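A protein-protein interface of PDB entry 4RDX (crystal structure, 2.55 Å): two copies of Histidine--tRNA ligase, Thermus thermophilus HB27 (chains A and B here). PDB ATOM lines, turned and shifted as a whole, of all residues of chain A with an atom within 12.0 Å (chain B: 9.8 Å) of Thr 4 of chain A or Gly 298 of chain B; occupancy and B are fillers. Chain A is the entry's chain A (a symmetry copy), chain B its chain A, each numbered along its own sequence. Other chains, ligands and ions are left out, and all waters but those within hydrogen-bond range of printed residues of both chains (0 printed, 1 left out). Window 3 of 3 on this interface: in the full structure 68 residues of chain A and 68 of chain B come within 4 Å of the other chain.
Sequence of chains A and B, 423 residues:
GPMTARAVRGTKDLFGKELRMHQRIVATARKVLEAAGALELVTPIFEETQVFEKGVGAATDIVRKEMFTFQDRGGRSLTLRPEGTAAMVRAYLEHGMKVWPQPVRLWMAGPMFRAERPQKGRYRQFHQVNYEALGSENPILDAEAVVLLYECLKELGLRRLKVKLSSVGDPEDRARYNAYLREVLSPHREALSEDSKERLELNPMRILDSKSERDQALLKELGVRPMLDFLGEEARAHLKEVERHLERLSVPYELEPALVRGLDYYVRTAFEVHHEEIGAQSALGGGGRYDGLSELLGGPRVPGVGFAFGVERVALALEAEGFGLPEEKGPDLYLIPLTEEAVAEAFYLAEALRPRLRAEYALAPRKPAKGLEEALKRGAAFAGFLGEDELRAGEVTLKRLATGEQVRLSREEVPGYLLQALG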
ATOM      1  N   THR A   4       0.759 -22.410  19.442  1.00  0.00           N
ATOM      2  CA  THR A   4      -0.668 -22.703  19.369  1.00  0.00           C
ATOM      3  C   THR A   4      -1.113 -23.387  20.669  1.00  0.00           C
ATOM      4  O   THR A   4      -2.304 -23.607  20.900  1.00  0.00           O
ATOM      5  CB  THR A   4      -1.010 -23.548  18.105  1.00  0.00           C
ATOM      6  OG1 THR A   4      -2.241 -23.094  17.525  1.00  0.00           O
ATOM      7  CG2 THR A   4      -1.102 -25.033  18.427  1.00  0.00           C
ATOM      8  N   ALA A   5      -0.136 -23.694  21.523  1.00  0.00           N
ATOM      9  CA  ALA A   5      -0.393 -24.278  22.839  1.00  0.00           C
ATOM     10  C   ALA A   5      -0.539 -23.203  23.914  1.00  0.00           C
ATOM     11  O   ALA A   5       0.314 -22.324  24.051  1.00  0.00           O
ATOM     12  CB  ALA A   5       0.714 -25.251  23.219  1.00  0.00           C
ATOM     13  N   ARG A   6      -1.618 -23.292  24.683  1.00  0.00           N
ATOM     14  CA  ARG A   6      -1.937 -22.277  25.676  1.00  0.00           C
ATOM     15  C   ARG A   6      -2.102 -22.898  27.056  1.00  0.00           C
ATOM     16  O   ARG A   6      -2.420 -24.082  27.182  1.00  0.00           O
ATOM     17  CB  ARG A   6      -3.237 -21.567  25.295  1.00  0.00           C
ATOM     18  CG  ARG A   6      -3.289 -21.062  23.861  1.00  0.00           C
ATOM     19  CD  ARG A   6      -2.510 -19.767  23.699  1.00  0.00           C
ATOM     20  NE  ARG A   6      -1.272 -19.946  22.945  1.00  0.00           N
ATOM     21  CZ  ARG A   6      -1.161 -19.743  21.637  1.00  0.00           C
ATOM     22  NH1 ARG A   6      -2.218 -19.356  20.934  1.00  0.00           N
ATOM     23  NH2 ARG A   6       0.006 -19.925  21.032  1.00  0.00           N
ATOM     24  N   ALA A   7      -1.878 -22.090  28.089  1.00  0.00           N
ATOM     25  CA  ALA A   7      -2.201 -22.480  29.451  1.00  0.00           C
ATOM     26  C   ALA A   7      -3.690 -22.789  29.500  1.00  0.00           C
ATOM     27  O   ALA A   7      -4.494 -22.083  28.888  1.00  0.00           O
ATOM     28  CB  ALA A   7      -1.858 -21.358  30.413  1.00  0.00           C
ATOM     29  N   VAL A   8      -4.059 -23.849  30.212  1.00  0.00           N
ATOM     30  CA  VAL A   8      -5.449 -24.298  30.226  1.00  0.00           C
ATOM     31  C   VAL A   8      -6.351 -23.311  30.961  1.00  0.00           C
ATOM     32  O   VAL A   8      -5.879 -22.500  31.760  1.00  0.00           O
ATOM     33  CB  VAL A   8      -5.589 -25.707  30.840  1.00  0.00           C
ATOM     34  CG1 VAL A   8      -4.457 -26.600  30.356  1.00  0.00           C
ATOM     35  CG2 VAL A   8      -5.602 -25.635  32.360  1.00  0.00           C
ATOM     36  N   ARG A   9      -7.646 -23.377  30.665  1.00  0.00           N
ATOM     37  CA  ARG A   9      -8.625 -22.491  31.277  1.00  0.00           C
ATOM     38  C   ARG A   9      -8.574 -22.590  32.795  1.00  0.00           C
ATOM     39  O   ARG A   9      -8.608 -23.685  33.354  1.00  0.00           O
ATOM     40  CB  ARG A   9     -10.033 -22.827  30.778  1.00  0.00           C
ATOM     41  CG  ARG A   9     -11.140 -22.361  31.712  1.00  0.00           C
ATOM     42  CD  ARG A   9     -12.438 -22.105  30.962  1.00  0.00           C
ATOM     43  NE  ARG A   9     -12.978 -23.315  30.346  1.00  0.00           N
ATOM     44  CZ  ARG A   9     -13.644 -23.330  29.195  1.00  0.00           C
ATOM     45  NH1 ARG A   9     -13.840 -22.202  28.526  1.00  0.00           N
ATOM     46  NH2 ARG A   9     -14.104 -24.475  28.708  1.00  0.00           N
ATOM     47  N   ASP A  13       0.123 -17.937  33.957  1.00  0.00           N
ATOM     48  CA  ASP A  13       1.519 -17.780  34.325  1.00  0.00           C
ATOM     49  C   ASP A  13       1.629 -16.569  35.246  1.00  0.00           C
ATOM     50  O   ASP A  13       0.725 -15.729  35.294  1.00  0.00           O
ATOM     51  CB  ASP A  13       2.397 -17.617  33.084  1.00  0.00           C
ATOM     52  CG  ASP A  13       2.411 -18.863  32.214  1.00  0.00           C
ATOM     53  OD1 ASP A  13       3.024 -19.870  32.628  1.00  0.00           O
ATOM     54  OD2 ASP A  13       1.812 -18.838  31.118  1.00  0.00           O
ATOM     55  N   GLU B  47      -0.271 -28.953  32.534  1.00  0.00           N
ATOM     56  CA  GLU B  47      -0.442 -28.335  31.224  1.00  0.00           C
ATOM     57  C   GLU B  47      -1.221 -29.304  30.355  1.00  0.00           C
ATOM     58  O   GLU B  47      -1.434 -30.445  30.752  1.00  0.00           O
ATOM     59  CB  GLU B  47       0.915 -28.025  30.591  1.00  0.00           C
ATOM     60  CG  GLU B  47       1.798 -27.109  31.422  1.00  0.00           C
ATOM     61  CD  GLU B  47       1.874 -25.704  30.864  1.00  0.00           C
ATOM     62  OE1 GLU B  47       1.191 -25.427  29.856  1.00  0.00           O
ATOM     63  OE2 GLU B  47       2.622 -24.878  31.429  1.00  0.00           O
ATOM     64  N   GLU B  48      -1.665 -28.865  29.182  1.00  0.00           N
ATOM     65  CA  GLU B  48      -2.261 -29.813  28.251  1.00  0.00           C
ATOM     66  C   GLU B  48      -1.184 -30.818  27.855  1.00  0.00           C
ATOM     67  O   GLU B  48      -0.013 -30.456  27.734  1.00  0.00           O
ATOM     68  CB  GLU B  48      -2.880 -29.117  27.035  1.00  0.00           C
ATOM     69  CG  GLU B  48      -2.163 -27.871  26.556  1.00  0.00           C
ATOM     70  CD  GLU B  48      -2.949 -27.150  25.473  1.00  0.00           C
ATOM     71  OE1 GLU B  48      -4.198 -27.210  25.511  1.00  0.00           O
ATOM     72  OE2 GLU B  48      -2.324 -26.536  24.580  1.00  0.00           O
ATOM     73  N   GLN B  50      -0.185 -32.301  25.246  1.00  0.00           N
ATOM     74  CA  GLN B  50       0.558 -32.044  24.011  1.00  0.00           C
ATOM     75  C   GLN B  50       1.923 -31.384  24.217  1.00  0.00           C
ATOM     76  O   GLN B  50       2.887 -31.720  23.524  1.00  0.00           O
ATOM     77  CB  GLN B  50      -0.283 -31.186  23.062  1.00  0.00           C
ATOM     78  CG  GLN B  50      -1.474 -31.908  22.457  1.00  0.00           C
ATOM     79  CD  GLN B  50      -1.059 -33.068  21.574  1.00  0.00           C
ATOM     80  OE1 GLN B  50      -1.094 -34.225  21.993  1.00  0.00           O
ATOM     81  NE2 GLN B  50      -0.659 -32.764  20.345  1.00  0.00           N
ATOM     82  N   VAL B  51       2.002 -30.457  25.169  1.00  0.00           N
ATOM     83  CA  VAL B  51       3.233 -29.705  25.415  1.00  0.00           C
ATOM     84  C   VAL B  51       4.379 -30.550  25.986  1.00  0.00           C
ATOM     85  O   VAL B  51       5.537 -30.139  25.923  1.00  0.00           O
ATOM     86  CB  VAL B  51       2.988 -28.418  26.293  1.00  0.00           C
ATOM     87  CG1 VAL B  51       1.517 -28.057  26.344  1.00  0.00           C
ATOM     88  CG2 VAL B  51       3.545 -28.579  27.705  1.00  0.00           C
ATOM     89  N   LYS B  54       6.913 -35.205  23.309  1.00  0.00           N
ATOM     90  CA  LYS B  54       7.739 -34.758  22.196  1.00  0.00           C
ATOM     91  C   LYS B  54       8.508 -35.916  21.572  1.00  0.00           C
ATOM     92  O   LYS B  54       8.646 -35.996  20.353  1.00  0.00           O
ATOM     93  CB  LYS B  54       8.706 -33.662  22.653  1.00  0.00           C
ATOM     94  CG  LYS B  54       8.071 -32.284  22.826  1.00  0.00           C
ATOM     95  CD  LYS B  54       7.334 -32.136  24.152  1.00  0.00           C
ATOM     96  CE  LYS B  54       8.250 -31.635  25.262  1.00  0.00           C
ATOM     97  NZ  LYS B  54       9.245 -32.649  25.704  1.00  0.00           N
ATOM     98  N   ARG B  76     -10.404 -33.218  28.022  1.00  0.00           N
ATOM     99  CA  ARG B  76      -9.045 -32.832  27.656  1.00  0.00           C
ATOM    100  C   ARG B  76      -7.989 -33.559  28.481  1.00  0.00           C
ATOM    101  O   ARG B  76      -8.112 -33.681  29.701  1.00  0.00           O
ATOM    102  CB  ARG B  76      -8.864 -31.322  27.797  1.00  0.00           C
ATOM    103  CG  ARG B  76      -7.482 -30.830  27.412  1.00  0.00           C
ATOM    104  CD  ARG B  76      -7.409 -29.320  27.506  1.00  0.00           C
ATOM    105  NE  ARG B  76      -8.491 -28.689  26.755  1.00  0.00           N
ATOM    106  CZ  ARG B  76      -8.642 -27.376  26.619  1.00  0.00           C
ATOM    107  NH1 ARG B  76      -7.778 -26.544  27.186  1.00  0.00           N
ATOM    108  NH2 ARG B  76      -9.659 -26.895  25.917  1.00  0.00           N
ATOM    109  N   ALA B  86       9.997 -26.998  28.503  1.00  0.00           N
ATOM    110  CA  ALA B  86       8.889 -26.910  27.558  1.00  0.00           C
ATOM    111  C   ALA B  86       7.827 -25.921  28.031  1.00  0.00           C
ATOM    112  O   ALA B  86       7.279 -25.156  27.237  1.00  0.00           O
ATOM    113  CB  ALA B  86       8.276 -28.280  27.331  1.00  0.00           C
ATOM    114  N   VAL B  89       9.055 -22.399  27.470  1.00  0.00           N
ATOM    115  CA  VAL B  89       8.958 -22.031  26.060  1.00  0.00           C
ATOM    116  C   VAL B  89       7.507 -21.722  25.688  1.00  0.00           C
ATOM    117  O   VAL B  89       7.232 -20.778  24.940  1.00  0.00           O
ATOM    118  CB  VAL B  89       9.528 -23.118  25.126  1.00  0.00           C
ATOM    119  CG1 VAL B  89       9.353 -22.709  23.670  1.00  0.00           C
ATOM    120  CG2 VAL B  89      10.995 -23.357  25.432  1.00  0.00           C
ATOM    121  N   ARG B  90       6.581 -22.513  26.222  1.00  0.00           N
ATOM    122  CA  ARG B  90       5.160 -22.248  26.022  1.00  0.00           C
ATOM    123  C   ARG B  90       4.808 -20.863  26.569  1.00  0.00           C
ATOM    124  O   ARG B  90       4.012 -20.138  25.976  1.00  0.00           O
ATOM    125  CB  ARG B  90       4.307 -23.334  26.686  1.00  0.00           C
ATOM    126  CG  ARG B  90       2.858 -23.400  26.199  1.00  0.00           C
ATOM    127  CD  ARG B  90       1.955 -22.462  26.983  1.00  0.00           C
ATOM    128  NE  ARG B  90       2.054 -22.700  28.418  1.00  0.00           N
ATOM    129  CZ  ARG B  90       2.101 -21.740  29.335  1.00  0.00           C
ATOM    130  NH1 ARG B  90       2.056 -20.467  28.969  1.00  0.00           N
ATOM    131  NH2 ARG B  90       2.195 -22.051  30.620  1.00  0.00           N
ATOM    132  N   ALA B  91       5.409 -20.505  27.701  1.00  0.00           N
ATOM    133  CA  ALA B  91       5.224 -19.177  28.284  1.00  0.00           C
ATOM    134  C   ALA B  91       5.797 -18.095  27.373  1.00  0.00           C
ATOM    135  O   ALA B  91       5.210 -17.022  27.219  1.00  0.00           O
ATOM    136  CB  ALA B  91       5.864 -19.108  29.656  1.00  0.00           C
ATOM    137  N   TYR B  92       6.955 -18.384  26.785  1.00  0.00           N
ATOM    138  CA  TYR B  92       7.578 -17.487  25.816  1.00  0.00           C
ATOM    139  C   TYR B  92       6.620 -17.203  24.661  1.00  0.00           C
ATOM    140  O   TYR B  92       6.448 -16.055  24.253  1.00  0.00           O
ATOM    141  CB  TYR B  92       8.885 -18.092  25.289  1.00  0.00           C
ATOM    142  CG  TYR B  92       9.606 -17.240  24.270  1.00  0.00           C
ATOM    143  CD1 TYR B  92       9.367 -17.395  22.907  1.00  0.00           C
ATOM    144  CD2 TYR B  92      10.535 -16.289  24.663  1.00  0.00           C
ATOM    145  CE1 TYR B  92      10.030 -16.620  21.968  1.00  0.00           C
ATOM    146  CE2 TYR B  92      11.194 -15.510  23.730  1.00  0.00           C
ATOM    147  CZ  TYR B  92      10.943 -15.678  22.389  1.00  0.00           C
ATOM    148  OH  TYR B  92      11.616 -14.894  21.478  1.00  0.00           O
ATOM    149  N   LEU B  93       5.988 -18.254  24.150  1.00  0.00           N
ATOM    150  CA  LEU B  93       5.064 -18.118  23.028  1.00  0.00           C
ATOM    151  C   LEU B  93       3.792 -17.366  23.412  1.00  0.00           C
ATOM    152  O   LEU B  93       3.374 -16.435  22.724  1.00  0.00           O
ATOM    153  CB  LEU B  93       4.694 -19.497  22.478  1.00  0.00           C
ATOM    154  CG  LEU B  93       5.473 -20.038  21.277  1.00  0.00           C
ATOM    155  CD1 LEU B  93       6.920 -19.569  21.293  1.00  0.00           C
ATOM    156  CD2 LEU B  93       5.402 -21.558  21.264  1.00  0.00           C
ATOM    157  N   GLU B  94       3.188 -17.782  24.520  1.00  0.00           N
ATOM    158  CA  GLU B  94       1.885 -17.275  24.940  1.00  0.00           C
ATOM    159  C   GLU B  94       1.875 -15.783  25.252  1.00  0.00           C
ATOM    160  O   GLU B  94       0.916 -15.083  24.931  1.00  0.00           O
ATOM    161  CB  GLU B  94       1.376 -18.062  26.151  1.00  0.00           C
ATOM    162  CG  GLU B  94       0.025 -17.597  26.661  1.00  0.00           C
ATOM    163  CD  GLU B  94      -0.783 -18.719  27.275  1.00  0.00           C
ATOM    164  OE1 GLU B  94      -0.231 -19.827  27.442  1.00  0.00           O
ATOM    165  OE2 GLU B  94      -1.972 -18.496  27.583  1.00  0.00           O
ATOM    166  N   LYS B  98       8.569 -12.595  21.966  1.00  0.00           N
ATOM    167  CA  LYS B  98       9.361 -12.374  20.762  1.00  0.00           C
ATOM    168  C   LYS B  98       9.593 -10.883  20.524  1.00  0.00           C
ATOM    169  O   LYS B  98      10.510 -10.502  19.798  1.00  0.00           O
ATOM    170  CB  LYS B  98       8.684 -13.017  19.542  1.00  0.00           C
ATOM    171  CG  LYS B  98       7.377 -12.356  19.117  1.00  0.00           C
ATOM    172  CD  LYS B  98       6.610 -13.225  18.127  1.00  0.00           C
ATOM    173  CE  LYS B  98       5.386 -12.503  17.583  1.00  0.00           C
ATOM    174  NZ  LYS B  98       4.489 -13.415  16.817  1.00  0.00           N
ATOM    175  N   GLY B 292      13.882 -26.562  17.950  1.00  0.00           N
ATOM    176  CA  GLY B 292      12.820 -27.386  17.403  1.00  0.00           C
ATOM    177  C   GLY B 292      11.659 -27.514  18.370  1.00  0.00           C
ATOM    178  O   GLY B 292      10.551 -27.878  17.981  1.00  0.00           O
ATOM    179  N   LEU B 293      11.923 -27.203  19.635  1.00  0.00           N
ATOM    180  CA  LEU B 293      10.930 -27.308  20.699  1.00  0.00           C
ATOM    181  C   LEU B 293       9.705 -26.428  20.445  1.00  0.00           C
ATOM    182  O   LEU B 293       8.568 -26.898  20.506  1.00  0.00           O
ATOM    183  CB  LEU B 293      11.578 -26.958  22.045  1.00  0.00           C
ATOM    184  CG  LEU B 293      10.833 -27.244  23.353  1.00  0.00           C
ATOM    185  CD1 LEU B 293      10.017 -28.518  23.242  1.00  0.00           C
ATOM    186  CD2 LEU B 293      11.825 -27.350  24.503  1.00  0.00           C
ATOM    187  N   SER B 294       9.945 -25.155  20.143  1.00  0.00           N
ATOM    188  CA  SER B 294       8.871 -24.183  19.962  1.00  0.00           C
ATOM    189  C   SER B 294       7.995 -24.468  18.739  1.00  0.00           C
ATOM    190  O   SER B 294       6.840 -24.042  18.689  1.00  0.00           O
ATOM    191  CB  SER B 294       9.441 -22.764  19.887  1.00  0.00           C
ATOM    192  OG  SER B 294      10.333 -22.632  18.796  1.00  0.00           O
ATOM    193  N   GLU B 295       8.541 -25.184  17.757  1.00  0.00           N
ATOM    194  CA  GLU B 295       7.774 -25.566  16.570  1.00  0.00           C
ATOM    195  C   GLU B 295       6.774 -26.679  16.883  1.00  0.00           C
ATOM    196  O   GLU B 295       5.644 -26.659  16.398  1.00  0.00           O
ATOM    197  CB  GLU B 295       8.697 -25.987  15.423  1.00  0.00           C
ATOM    198  CG  GLU B 295       9.416 -24.842  14.723  1.00  0.00           C
ATOM    199  CD  GLU B 295      10.784 -24.562  15.313  1.00  0.00           C
ATOM    200  OE1 GLU B 295      10.987 -24.859  16.510  1.00  0.00           O
ATOM    201  OE2 GLU B 295      11.662 -24.058  14.579  1.00  0.00           O
ATOM    202  N   LEU B 296       7.194 -27.642  17.700  1.00  0.00           N
ATOM    203  CA  LEU B 296       6.292 -28.677  18.190  1.00  0.00           C
ATOM    204  C   LEU B 296       5.227 -28.061  19.097  1.00  0.00           C
ATOM    205  O   LEU B 296       4.150 -28.633  19.282  1.00  0.00           O
ATOM    206  CB  LEU B 296       7.063 -29.778  18.924  1.00  0.00           C
ATOM    207  CG  LEU B 296       7.830 -30.769  18.041  1.00  0.00           C
ATOM    208  CD1 LEU B 296       9.322 -30.760  18.340  1.00  0.00           C
ATOM    209  CD2 LEU B 296       7.267 -32.179  18.181  1.00  0.00           C
ATOM    210  N   LEU B 297       5.537 -26.894  19.657  1.00  0.00           N
ATOM    211  CA  LEU B 297       4.580 -26.141  20.460  1.00  0.00           C
ATOM    212  C   LEU B 297       3.727 -25.240  19.570  1.00  0.00           C
ATOM    213  O   LEU B 297       2.851 -24.521  20.050  1.00  0.00           O
ATOM    214  CB  LEU B 297       5.302 -25.320  21.531  1.00  0.00           C
ATOM    215  CG  LEU B 297       5.956 -26.123  22.657  1.00  0.00           C
ATOM    216  CD1 LEU B 297       6.748 -25.209  23.575  1.00  0.00           C
ATOM    217  CD2 LEU B 297       4.901 -26.886  23.441  1.00  0.00           C
ATOM    218  N   GLY B 298       3.995 -25.288  18.268  1.00  0.00           N
ATOM    219  CA  GLY B 298       3.171 -24.608  17.284  1.00  0.00           C
ATOM    220  C   GLY B 298       3.641 -23.217  16.906  1.00  0.00           C
ATOM    221  O   GLY B 298       2.957 -22.508  16.168  1.00  0.00           O
ATOM    222  N   GLY B 299       4.805 -22.821  17.408  1.00  0.00           N
ATOM    223  CA  GLY B 299       5.338 -21.500  17.130  1.00  0.00           C
ATOM    224  C   GLY B 299       6.426 -21.515  16.074  1.00  0.00           C
ATOM    225  O   GLY B 299       6.607 -22.517  15.379  1.00  0.00           O
ATOM    226  N   PRO B 300       7.154 -20.397  15.943  1.00  0.00           N
ATOM    227  CA  PRO B 300       8.271 -20.278  15.003  1.00  0.00           C
ATOM    228  C   PRO B 300       9.552 -20.837  15.604  1.00  0.00           C
ATOM    229  O   PRO B 300       9.498 -21.565  16.600  1.00  0.00           O
ATOM    230  CB  PRO B 300       8.398 -18.769  14.822  1.00  0.00           C
ATOM    231  CG  PRO B 300       7.998 -18.221  16.148  1.00  0.00           C
ATOM    232  CD  PRO B 300       6.918 -19.139  16.673  1.00  0.00           C
ATOM    233  N   ARG B 301      10.690 -20.499  15.007  1.00  0.00           N
ATOM    234  CA  ARG B 301      11.980 -20.985  15.490  1.00  0.00           C
ATOM    235  C   ARG B 301      12.530 -20.101  16.603  1.00  0.00           C
ATOM    236  O   ARG B 301      12.876 -18.952  16.393  1.00  0.00           O
ATOM    237  CB  ARG B 301      13.002 -21.080  14.352  1.00  0.00           C
ATOM    238  CG  ARG B 301      14.386 -21.533  14.806  1.00  0.00           C
ATOM    239  CD  ARG B 301      15.364 -21.545  13.647  1.00  0.00           C
ATOM    240  NE  ARG B 301      16.557 -22.332  13.940  1.00  0.00           N
ATOM    241  CZ  ARG B 301      17.750 -21.815  14.212  1.00  0.00           C
ATOM    242  NH1 ARG B 301      17.922 -20.500  14.226  1.00  0.00           N
ATOM    243  NH2 ARG B 301      18.775 -22.618  14.464  1.00  0.00           N
ATOM    244  N   VAL B 302      12.596 -20.666  17.799  1.00  0.00           N
ATOM    245  CA  VAL B 302      13.194 -19.993  18.941  1.00  0.00           C
ATOM    246  C   VAL B 302      14.314 -20.878  19.463  1.00  0.00           C
ATOM    247  O   VAL B 302      14.034 -21.888  20.093  1.00  0.00           O
ATOM    248  CB  VAL B 302      12.180 -19.794  20.048  1.00  0.00           C
ATOM    249  CG1 VAL B 302      12.789 -19.054  21.210  1.00  0.00           C
ATOM    250  CG2 VAL B 302      10.931 -19.072  19.543  1.00  0.00           C
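Among the printed residues, pairs that only touch across the chains: Thr 4 of chain A with Gly 298 of chain B (3.9 Å), Ala 5 of chain A with Glu 48 of chain B (3.4 Å), Ala 5 of chain A with Arg 90 of chain B (3.4 Å), Arg 6 of chain A with Glu 94 of chain B (3.5 Å), Ala 7 of chain A with Arg 90 of chain B (3.99 Å) and Val 8 of chain A with Glu 48 of chain B (3.8 Å).
OE1 of Glu 94 of chain B sits at hydrogen-bond distance from N of Ala 7 of chain A, 2.9 Å away.
The backbone NH (N) of Thr 4 of chain A sits at hydrogen-bond distance from the backbone carbonyl oxygen (O) of Leu 297 of chain B, 3.0 Å away.
The backbone carbonyl oxygen (O) of Leu 297 of chain B sits at hydrogen-bond distance from the backbone NH (N) of Ala 5 of chain A, at 3.4 Å.
OE2 of Glu 48 of chain B lies within hydrogen-bond range of N of Arg 6 of chain A (3.3 Å).
The guanidinium group (NH1) of Arg 90 of chain B is in salt-bridge range of the side-chain carboxylate (OD2) of Asp 13 of chain A.
Thr 4 of chain A touches just these residues of chain B: Leu 297 (3.0 Å) and Gly 298 (3.9 Å).
Printed residues of chain B within 4 Å of Ala 5 of chain A: Glu 48, Arg 90 and Leu 297.
Printed residues of chain B within 4 Å of Val 8 of chain A: Glu 48.
Printed residues of chain B within 4 Å of Asp 13 of chain A: Arg 90 (2.7 Å).
Of the printed residues of chain A, Glu 48 of chain B touches Ala 5, Arg 6 and Val 8.
Printed residues of chain A within 4 Å of Arg 90 of chain B: Ala 5, Ala 7 and Asp 13.
No residue of chain A comes within 4 Å of Leu 296 of chain B.
Of chain A, only Thr 4 (3.0 Å) and Ala 5 (3.4 Å) come within 4 Å of Leu 297 of chain B.
Printed residues of chain A within 4 Å of Gly 298 of chain B: Thr 4 (3.9 Å).
No residue of chain A comes within 4 Å of Gly 299 of chain B.
No residue of chain A comes within 4 Å of Pro 300 of chain B.
The nearest residue of chain B that does not touch Thr 4 of chain A is Gly 299 of chain B (4.5 Å).
The nearest residue of chain A that does not touch Gly 298 of chain B is Ala 5 of chain A (5.5 Å).
NH1 of Arg 90 of chain B is in salt-bridge range of OE1 of Glu 94 of chain B (2.8 Å).
The side-chain carboxylate of Glu 47 of chain B lies within salt-bridge range of the guanidinium group of Arg 90 of chain B, at 3.0 Å.
Of the 7 printed residues of chain A, 6 touch a printed residue of chain B.
Hydrophobic or aromatic side chains of chain A within 4 Å of the printed part of chain B: Ala 5, Ala 7 and Val 8.
Of the 25 printed residues of chain B, 5 touch a printed residue of chain A.
Along chain B the printed residues that touch a printed residue of chain A span positions 48 to 298.
No position is printed for both chains.
Of the 11 pairs that touch across the chains among the printed residues, none has its exchanged pair printed and touching as well.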
